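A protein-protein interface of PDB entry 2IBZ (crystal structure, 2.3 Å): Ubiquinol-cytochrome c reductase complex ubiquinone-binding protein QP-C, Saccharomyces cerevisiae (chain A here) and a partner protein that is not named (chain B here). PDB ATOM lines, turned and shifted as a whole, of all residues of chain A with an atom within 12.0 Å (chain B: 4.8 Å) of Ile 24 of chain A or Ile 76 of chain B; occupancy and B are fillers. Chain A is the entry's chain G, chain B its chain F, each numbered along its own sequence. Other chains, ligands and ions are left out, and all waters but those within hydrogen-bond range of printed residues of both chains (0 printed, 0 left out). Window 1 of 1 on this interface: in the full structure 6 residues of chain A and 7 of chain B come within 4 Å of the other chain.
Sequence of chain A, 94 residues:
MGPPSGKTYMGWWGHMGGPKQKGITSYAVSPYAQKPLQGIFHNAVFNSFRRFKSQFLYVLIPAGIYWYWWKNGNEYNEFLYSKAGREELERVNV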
ATOM      1  N   TRP A  13     -33.874 -23.270  -8.387  1.00  0.00           N
ATOM      2  CA  TRP A  13     -33.296 -24.447  -7.733  1.00  0.00           C
ATOM      3  C   TRP A  13     -32.685 -25.431  -8.724  1.00  0.00           C
ATOM      4  O   TRP A  13     -33.379 -25.938  -9.622  1.00  0.00           O
ATOM      5  CB  TRP A  13     -34.364 -25.146  -6.900  1.00  0.00           C
ATOM      6  CG  TRP A  13     -34.959 -24.237  -5.886  1.00  0.00           C
ATOM      7  CD1 TRP A  13     -36.207 -23.704  -5.902  1.00  0.00           C
ATOM      8  CD2 TRP A  13     -34.326 -23.755  -4.696  1.00  0.00           C
ATOM      9  NE1 TRP A  13     -36.399 -22.918  -4.792  1.00  0.00           N
ATOM     10  CE2 TRP A  13     -35.263 -22.935  -4.030  1.00  0.00           C
ATOM     11  CE3 TRP A  13     -33.058 -23.943  -4.123  1.00  0.00           C
ATOM     12  CZ2 TRP A  13     -34.978 -22.299  -2.804  1.00  0.00           C
ATOM     13  CZ3 TRP A  13     -32.769 -23.315  -2.901  1.00  0.00           C
ATOM     14  CH2 TRP A  13     -33.728 -22.505  -2.255  1.00  0.00           C
ATOM     15  N   MET A  16     -29.206 -21.963 -10.091  1.00  0.00           N
ATOM     16  CA  MET A  16     -29.298 -20.623  -9.525  1.00  0.00           C
ATOM     17  C   MET A  16     -28.467 -19.572 -10.229  1.00  0.00           C
ATOM     18  O   MET A  16     -28.807 -18.385 -10.188  1.00  0.00           O
ATOM     19  CB  MET A  16     -28.959 -20.635  -8.036  1.00  0.00           C
ATOM     20  CG  MET A  16     -29.698 -19.569  -7.239  1.00  0.00           C
ATOM     21  SD  MET A  16     -31.485 -19.847  -7.218  1.00  0.00           S
ATOM     22  CE  MET A  16     -31.598 -21.178  -6.018  1.00  0.00           C
ATOM     23  N   GLY A  17     -27.392 -20.006 -10.884  1.00  0.00           N
ATOM     24  CA  GLY A  17     -26.535 -19.074 -11.591  1.00  0.00           C
ATOM     25  C   GLY A  17     -25.267 -18.701 -10.835  1.00  0.00           C
ATOM     26  O   GLY A  17     -24.524 -17.807 -11.253  1.00  0.00           O
ATOM     27  N   GLY A  18     -25.047 -19.346  -9.696  1.00  0.00           N
ATOM     28  CA  GLY A  18     -23.849 -19.094  -8.927  1.00  0.00           C
ATOM     29  C   GLY A  18     -22.700 -19.877  -9.533  1.00  0.00           C
ATOM     30  O   GLY A  18     -22.888 -20.602 -10.520  1.00  0.00           O
ATOM     31  N   PRO A  19     -21.484 -19.733  -8.987  1.00  0.00           N
ATOM     32  CA  PRO A  19     -20.326 -20.464  -9.515  1.00  0.00           C
ATOM     33  C   PRO A  19     -20.407 -21.901  -9.001  1.00  0.00           C
ATOM     34  O   PRO A  19     -21.124 -22.167  -8.029  1.00  0.00           O
ATOM     35  CB  PRO A  19     -19.151 -19.718  -8.880  1.00  0.00           C
ATOM     36  CG  PRO A  19     -19.687 -19.390  -7.501  1.00  0.00           C
ATOM     37  CD  PRO A  19     -21.093 -18.878  -7.845  1.00  0.00           C
ATOM     38  N   LYS A  20     -19.679 -22.819  -9.633  1.00  0.00           N
ATOM     39  CA  LYS A  20     -19.682 -24.217  -9.200  1.00  0.00           C
ATOM     40  C   LYS A  20     -19.068 -24.358  -7.808  1.00  0.00           C
ATOM     41  O   LYS A  20     -17.974 -23.885  -7.560  1.00  0.00           O
ATOM     42  CB  LYS A  20     -18.943 -25.095 -10.211  1.00  0.00           C
ATOM     43  CG  LYS A  20     -19.502 -24.986 -11.620  1.00  0.00           C
ATOM     44  CD  LYS A  20     -19.268 -26.239 -12.436  1.00  0.00           C
ATOM     45  CE  LYS A  20     -19.625 -26.012 -13.917  1.00  0.00           C
ATOM     46  NZ  LYS A  20     -20.987 -25.391 -14.126  1.00  0.00           N
ATOM     47  N   GLN A  21     -19.799 -24.964  -6.885  1.00  0.00           N
ATOM     48  CA  GLN A  21     -19.317 -25.130  -5.518  1.00  0.00           C
ATOM     49  C   GLN A  21     -18.704 -26.505  -5.318  1.00  0.00           C
ATOM     50  O   GLN A  21     -19.240 -27.498  -5.792  1.00  0.00           O
ATOM     51  CB  GLN A  21     -20.461 -24.919  -4.514  1.00  0.00           C
ATOM     52  CG  GLN A  21     -21.054 -23.514  -4.506  1.00  0.00           C
ATOM     53  CD  GLN A  21     -22.164 -23.360  -3.478  1.00  0.00           C
ATOM     54  OE1 GLN A  21     -22.188 -24.070  -2.477  1.00  0.00           O
ATOM     55  NE2 GLN A  21     -23.089 -22.432  -3.721  1.00  0.00           N
ATOM     56  N   LYS A  22     -17.582 -26.551  -4.608  1.00  0.00           N
ATOM     57  CA  LYS A  22     -16.875 -27.799  -4.327  1.00  0.00           C
ATOM     58  C   LYS A  22     -16.026 -27.570  -3.078  1.00  0.00           C
ATOM     59  O   LYS A  22     -15.472 -26.486  -2.900  1.00  0.00           O
ATOM     60  CB  LYS A  22     -15.967 -28.154  -5.501  1.00  0.00           C
ATOM     61  CG  LYS A  22     -15.318 -29.534  -5.425  1.00  0.00           C
ATOM     62  CD  LYS A  22     -14.359 -29.734  -6.614  1.00  0.00           C
ATOM     63  CE  LYS A  22     -14.168 -31.207  -6.978  1.00  0.00           C
ATOM     64  NZ  LYS A  22     -13.768 -32.021  -5.808  1.00  0.00           N
ATOM     65  N   GLY A  23     -15.965 -28.562  -2.195  1.00  0.00           N
ATOM     66  CA  GLY A  23     -15.171 -28.433  -0.991  1.00  0.00           C
ATOM     67  C   GLY A  23     -15.868 -27.918   0.252  1.00  0.00           C
ATOM     68  O   GLY A  23     -15.332 -28.036   1.357  1.00  0.00           O
ATOM     69  N   ILE A  24     -17.032 -27.299   0.083  1.00  0.00           N
ATOM     70  CA  ILE A  24     -17.790 -26.769   1.219  1.00  0.00           C
ATOM     71  C   ILE A  24     -18.772 -27.843   1.690  1.00  0.00           C
ATOM     72  O   ILE A  24     -19.507 -28.408   0.886  1.00  0.00           O
ATOM     73  CB  ILE A  24     -18.584 -25.510   0.805  1.00  0.00           C
ATOM     74  CG1 ILE A  24     -17.635 -24.471   0.200  1.00  0.00           C
ATOM     75  CG2 ILE A  24     -19.365 -24.955   2.000  1.00  0.00           C
ATOM     76  CD1 ILE A  24     -18.317 -23.403  -0.629  1.00  0.00           C
ATOM     77  N   THR A  25     -18.776 -28.116   2.989  1.00  0.00           N
ATOM     78  CA  THR A  25     -19.657 -29.112   3.578  1.00  0.00           C
ATOM     79  C   THR A  25     -20.442 -28.427   4.689  1.00  0.00           C
ATOM     80  O   THR A  25     -19.845 -27.786   5.557  1.00  0.00           O
ATOM     81  CB  THR A  25     -18.820 -30.286   4.178  1.00  0.00           C
ATOM     82  OG1 THR A  25     -18.109 -30.937   3.122  1.00  0.00           O
ATOM     83  CG2 THR A  25     -19.695 -31.304   4.897  1.00  0.00           C
ATOM     84  N   SER A  26     -21.769 -28.551   4.676  1.00  0.00           N
ATOM     85  CA  SER A  26     -22.568 -27.906   5.712  1.00  0.00           C
ATOM     86  C   SER A  26     -23.223 -28.907   6.631  1.00  0.00           C
ATOM     87  O   SER A  26     -23.458 -30.045   6.256  1.00  0.00           O
ATOM     88  CB  SER A  26     -23.619 -26.964   5.105  1.00  0.00           C
ATOM     89  OG  SER A  26     -24.592 -27.671   4.360  1.00  0.00           O
ATOM     90  N   TYR A  27     -23.520 -28.475   7.844  1.00  0.00           N
ATOM     91  CA  TYR A  27     -24.147 -29.350   8.821  1.00  0.00           C
ATOM     92  C   TYR A  27     -25.241 -28.578   9.522  1.00  0.00           C
ATOM     93  O   TYR A  27     -25.102 -27.373   9.738  1.00  0.00           O
ATOM     94  CB  TYR A  27     -23.132 -29.789   9.887  1.00  0.00           C
ATOM     95  CG  TYR A  27     -21.904 -30.505   9.371  1.00  0.00           C
ATOM     96  CD1 TYR A  27     -20.812 -29.790   8.873  1.00  0.00           C
ATOM     97  CD2 TYR A  27     -21.802 -31.896   9.446  1.00  0.00           C
ATOM     98  CE1 TYR A  27     -19.655 -30.442   8.466  1.00  0.00           C
ATOM     99  CE2 TYR A  27     -20.643 -32.557   9.048  1.00  0.00           C
ATOM    100  CZ  TYR A  27     -19.575 -31.828   8.563  1.00  0.00           C
ATOM    101  OH  TYR A  27     -18.415 -32.479   8.192  1.00  0.00           O
ATOM    102  N   ALA A  28     -26.300 -29.273   9.921  1.00  0.00           N
ATOM    103  CA  ALA A  28     -27.394 -28.636  10.635  1.00  0.00           C
ATOM    104  C   ALA A  28     -28.101 -29.672  11.513  1.00  0.00           C
ATOM    105  O   ALA A  28     -27.983 -30.875  11.287  1.00  0.00           O
ATOM    106  CB  ALA A  28     -28.386 -27.978   9.647  1.00  0.00           C
ATOM    107  N   TYR B  69     -13.388 -21.429  -5.844  1.00  0.00           N
ATOM    108  CA  TYR B  69     -14.000 -22.175  -4.743  1.00  0.00           C
ATOM    109  C   TYR B  69     -13.807 -21.410  -3.436  1.00  0.00           C
ATOM    110  O   TYR B  69     -14.659 -21.462  -2.549  1.00  0.00           O
ATOM    111  CB  TYR B  69     -13.387 -23.579  -4.598  1.00  0.00           C
ATOM    112  CG  TYR B  69     -13.523 -24.490  -5.803  1.00  0.00           C
ATOM    113  CD1 TYR B  69     -12.477 -25.336  -6.176  1.00  0.00           C
ATOM    114  CD2 TYR B  69     -14.697 -24.515  -6.570  1.00  0.00           C
ATOM    115  CE1 TYR B  69     -12.592 -26.181  -7.273  1.00  0.00           C
ATOM    116  CE2 TYR B  69     -14.820 -25.356  -7.671  1.00  0.00           C
ATOM    117  CZ  TYR B  69     -13.765 -26.187  -8.017  1.00  0.00           C
ATOM    118  OH  TYR B  69     -13.870 -27.028  -9.102  1.00  0.00           O
ATOM    119  N   ALA B  72     -16.239 -18.528  -3.160  1.00  0.00           N
ATOM    120  CA  ALA B  72     -17.543 -19.126  -2.857  1.00  0.00           C
ATOM    121  C   ALA B  72     -17.716 -19.395  -1.365  1.00  0.00           C
ATOM    122  O   ALA B  72     -18.759 -19.078  -0.779  1.00  0.00           O
ATOM    123  CB  ALA B  72     -17.738 -20.417  -3.657  1.00  0.00           C
ATOM    124  N   TYR B  73     -16.691 -19.977  -0.752  1.00  0.00           N
ATOM    125  CA  TYR B  73     -16.738 -20.259   0.677  1.00  0.00           C
ATOM    126  C   TYR B  73     -16.796 -18.974   1.500  1.00  0.00           C
ATOM    127  O   TYR B  73     -17.550 -18.891   2.472  1.00  0.00           O
ATOM    128  CB  TYR B  73     -15.525 -21.098   1.117  1.00  0.00           C
ATOM    129  CG  TYR B  73     -15.487 -21.327   2.604  1.00  0.00           C
ATOM    130  CD1 TYR B  73     -16.517 -22.011   3.245  1.00  0.00           C
ATOM    131  CD2 TYR B  73     -14.461 -20.794   3.389  1.00  0.00           C
ATOM    132  CE1 TYR B  73     -16.536 -22.156   4.632  1.00  0.00           C
ATOM    133  CE2 TYR B  73     -14.472 -20.932   4.783  1.00  0.00           C
ATOM    134  CZ  TYR B  73     -15.513 -21.612   5.395  1.00  0.00           C
ATOM    135  OH  TYR B  73     -15.548 -21.751   6.769  1.00  0.00           O
ATOM    136  N   ARG B  74     -15.993 -17.981   1.124  1.00  0.00           N
ATOM    137  CA  ARG B  74     -15.966 -16.718   1.860  1.00  0.00           C
ATOM    138  C   ARG B  74     -17.314 -16.010   1.819  1.00  0.00           C
ATOM    139  O   ARG B  74     -17.791 -15.500   2.842  1.00  0.00           O
ATOM    140  CB  ARG B  74     -14.852 -15.796   1.350  1.00  0.00           C
ATOM    141  CG  ARG B  74     -13.445 -16.280   1.669  1.00  0.00           C
ATOM    142  CD  ARG B  74     -12.416 -15.166   1.490  1.00  0.00           C
ATOM    143  NE  ARG B  74     -12.396 -14.630   0.126  1.00  0.00           N
ATOM    144  CZ  ARG B  74     -11.698 -15.145  -0.879  1.00  0.00           C
ATOM    145  NH1 ARG B  74     -11.756 -14.587  -2.081  1.00  0.00           N
ATOM    146  NH2 ARG B  74     -10.938 -16.210  -0.682  1.00  0.00           N
ATOM    147  N   ILE B  75     -17.940 -16.020   0.644  1.00  0.00           N
ATOM    148  CA  ILE B  75     -19.250 -15.403   0.460  1.00  0.00           C
ATOM    149  C   ILE B  75     -20.338 -16.127   1.280  1.00  0.00           C
ATOM    150  O   ILE B  75     -21.131 -15.495   2.004  1.00  0.00           O
ATOM    151  CB  ILE B  75     -19.609 -15.344  -1.037  1.00  0.00           C
ATOM    152  CG1 ILE B  75     -18.701 -14.316  -1.729  1.00  0.00           C
ATOM    153  CG2 ILE B  75     -21.092 -14.986  -1.230  1.00  0.00           C
ATOM    154  CD1 ILE B  75     -18.793 -14.313  -3.242  1.00  0.00           C
ATOM    155  N   ILE B  76     -20.337 -17.455   1.220  1.00  0.00           N
ATOM    156  CA  ILE B  76     -21.322 -18.221   1.977  1.00  0.00           C
ATOM    157  C   ILE B  76     -21.128 -18.007   3.471  1.00  0.00           C
ATOM    158  O   ILE B  76     -22.087 -17.753   4.205  1.00  0.00           O
ATOM    159  CB  ILE B  76     -21.279 -19.723   1.637  1.00  0.00           C
ATOM    160  CG1 ILE B  76     -21.699 -19.932   0.183  1.00  0.00           C
ATOM    161  CG2 ILE B  76     -22.205 -20.500   2.548  1.00  0.00           C
ATOM    162  CD1 ILE B  76     -21.547 -21.351  -0.303  1.00  0.00           C
ATOM    163  N   ARG B  77     -19.878 -18.047   3.911  1.00  0.00           N
ATOM    164  CA  ARG B  77     -19.553 -17.847   5.330  1.00  0.00           C
ATOM    165  C   ARG B  77     -19.981 -16.445   5.809  1.00  0.00           C
ATOM    166  O   ARG B  77     -20.474 -16.279   6.926  1.00  0.00           O
ATOM    167  CB  ARG B  77     -18.054 -18.093   5.555  1.00  0.00           C
ATOM    168  CG  ARG B  77     -17.572 -17.972   6.978  1.00  0.00           C
ATOM    169  CD  ARG B  77     -16.339 -17.084   6.998  1.00  0.00           C
ATOM    170  NE  ARG B  77     -15.079 -17.818   7.064  1.00  0.00           N
ATOM    171  CZ  ARG B  77     -13.944 -17.449   6.479  1.00  0.00           C
ATOM    172  NH1 ARG B  77     -12.866 -18.200   6.643  1.00  0.00           N
ATOM    173  NH2 ARG B  77     -13.888 -16.380   5.691  1.00  0.00           N
ATOM    174  N   ALA B  78     -19.832 -15.447   4.942  1.00  0.00           N
ATOM    175  CA  ALA B  78     -20.240 -14.083   5.285  1.00  0.00           C
ATOM    176  C   ALA B  78     -21.774 -13.979   5.459  1.00  0.00           C
ATOM    177  O   ALA B  78     -22.252 -13.325   6.399  1.00  0.00           O
ATOM    178  CB  ALA B  78     -19.742 -13.091   4.226  1.00  0.00           C
ATOM    179  N   HIS B  79     -22.543 -14.619   4.569  1.00  0.00           N
ATOM    180  CA  HIS B  79     -24.005 -14.577   4.689  1.00  0.00           C
ATOM    181  C   HIS B  79     -24.493 -15.232   5.969  1.00  0.00           C
ATOM    182  O   HIS B  79     -25.370 -14.686   6.652  1.00  0.00           O
ATOM    183  CB  HIS B  79     -24.697 -15.215   3.480  1.00  0.00           C
ATOM    184  CG  HIS B  79     -24.759 -14.319   2.283  1.00  0.00           C
ATOM    185  ND1 HIS B  79     -24.050 -14.566   1.126  1.00  0.00           N
ATOM    186  CD2 HIS B  79     -25.458 -13.181   2.061  1.00  0.00           C
ATOM    187  CE1 HIS B  79     -24.313 -13.622   0.241  1.00  0.00           C
ATOM    188  NE2 HIS B  79     -25.167 -12.769   0.783  1.00  0.00           N
ATOM    189  N   GLN B  80     -23.919 -16.391   6.294  1.00  0.00           N
ATOM    190  CA  GLN B  80     -24.288 -17.116   7.504  1.00  0.00           C
ATOM    191  C   GLN B  80     -23.964 -16.313   8.761  1.00  0.00           C
ATOM    192  O   GLN B  80     -24.769 -16.255   9.695  1.00  0.00           O
ATOM    193  CB  GLN B  80     -23.578 -18.465   7.566  1.00  0.00           C
ATOM    194  CG  GLN B  80     -23.884 -19.236   8.834  1.00  0.00           C
ATOM    195  CD  GLN B  80     -25.345 -19.646   8.937  1.00  0.00           C
ATOM    196  OE1 GLN B  80     -26.014 -19.875   7.924  1.00  0.00           O
ATOM    197  NE2 GLN B  80     -25.847 -19.743  10.160  1.00  0.00           N
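Tyr 69 of chain B touches Lys 20 of chain A. Gln 21 of chain A touches Ile 76 of chain B (OE1 to CD1, 3.5 Å). Lys 22 of chain A touches Tyr 69 of chain B. Tyr 73 of chain B touches Ile 24 of chain A (CA to CD1, 3.8 Å). Ile 76 of chain B touches Ile 24 of chain A.
Met 16 of chain A touches none of the printed residues of chain B. Pro 19 of chain A touches none of the printed residues of chain B. Of the printed residues of chain B, Gln 21 of chain A touches Ile 76 (3.5 Å). Printed residues of chain B within 4 Å of Lys 22 of chain A: Tyr 69. Printed residues of chain B within 4 Å of Ile 24 of chain A: Tyr 73 and Ile 76. Of the printed residues of chain A, Tyr 69 of chain B touches Lys 20 and Lys 22. No residue of chain A comes within 4 Å of Ala 72 of chain B. No residue of chain A comes within 4 Å of Ile 75 of chain B. Ile 76 of chain B touches just these residues of chain A: Gln 21 and Ile 24. Ala 78 of chain B touches none of the printed residues of chain A. No residue of chain A comes within 4 Å of His 79 of chain B. No residue of chain A comes within 4 Å of Gln 80 of chain B. The nearest residue of chain B that does not touch Ile 24 of chain A is Ala 72 of chain B (4.1 Å). The nearest printed residue of chain B that does not touch Lys 22 of chain A is Ala 72 of chain B (6.2 Å).
Of the 14 printed residues of chain A, 4 touch a printed residue of chain B. Hydrophobic or aromatic side chains of chain A that line the printed part of chain B: Ile 24. Hydrophobic or aromatic side chains of chain B within 4 Å of the printed part of chain A: Tyr 69 and Ile 76. Among the printed residues, no Asp or Glu carboxylate lies within 4 Å of a Lys or Arg side-chain nitrogen of the other chain.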
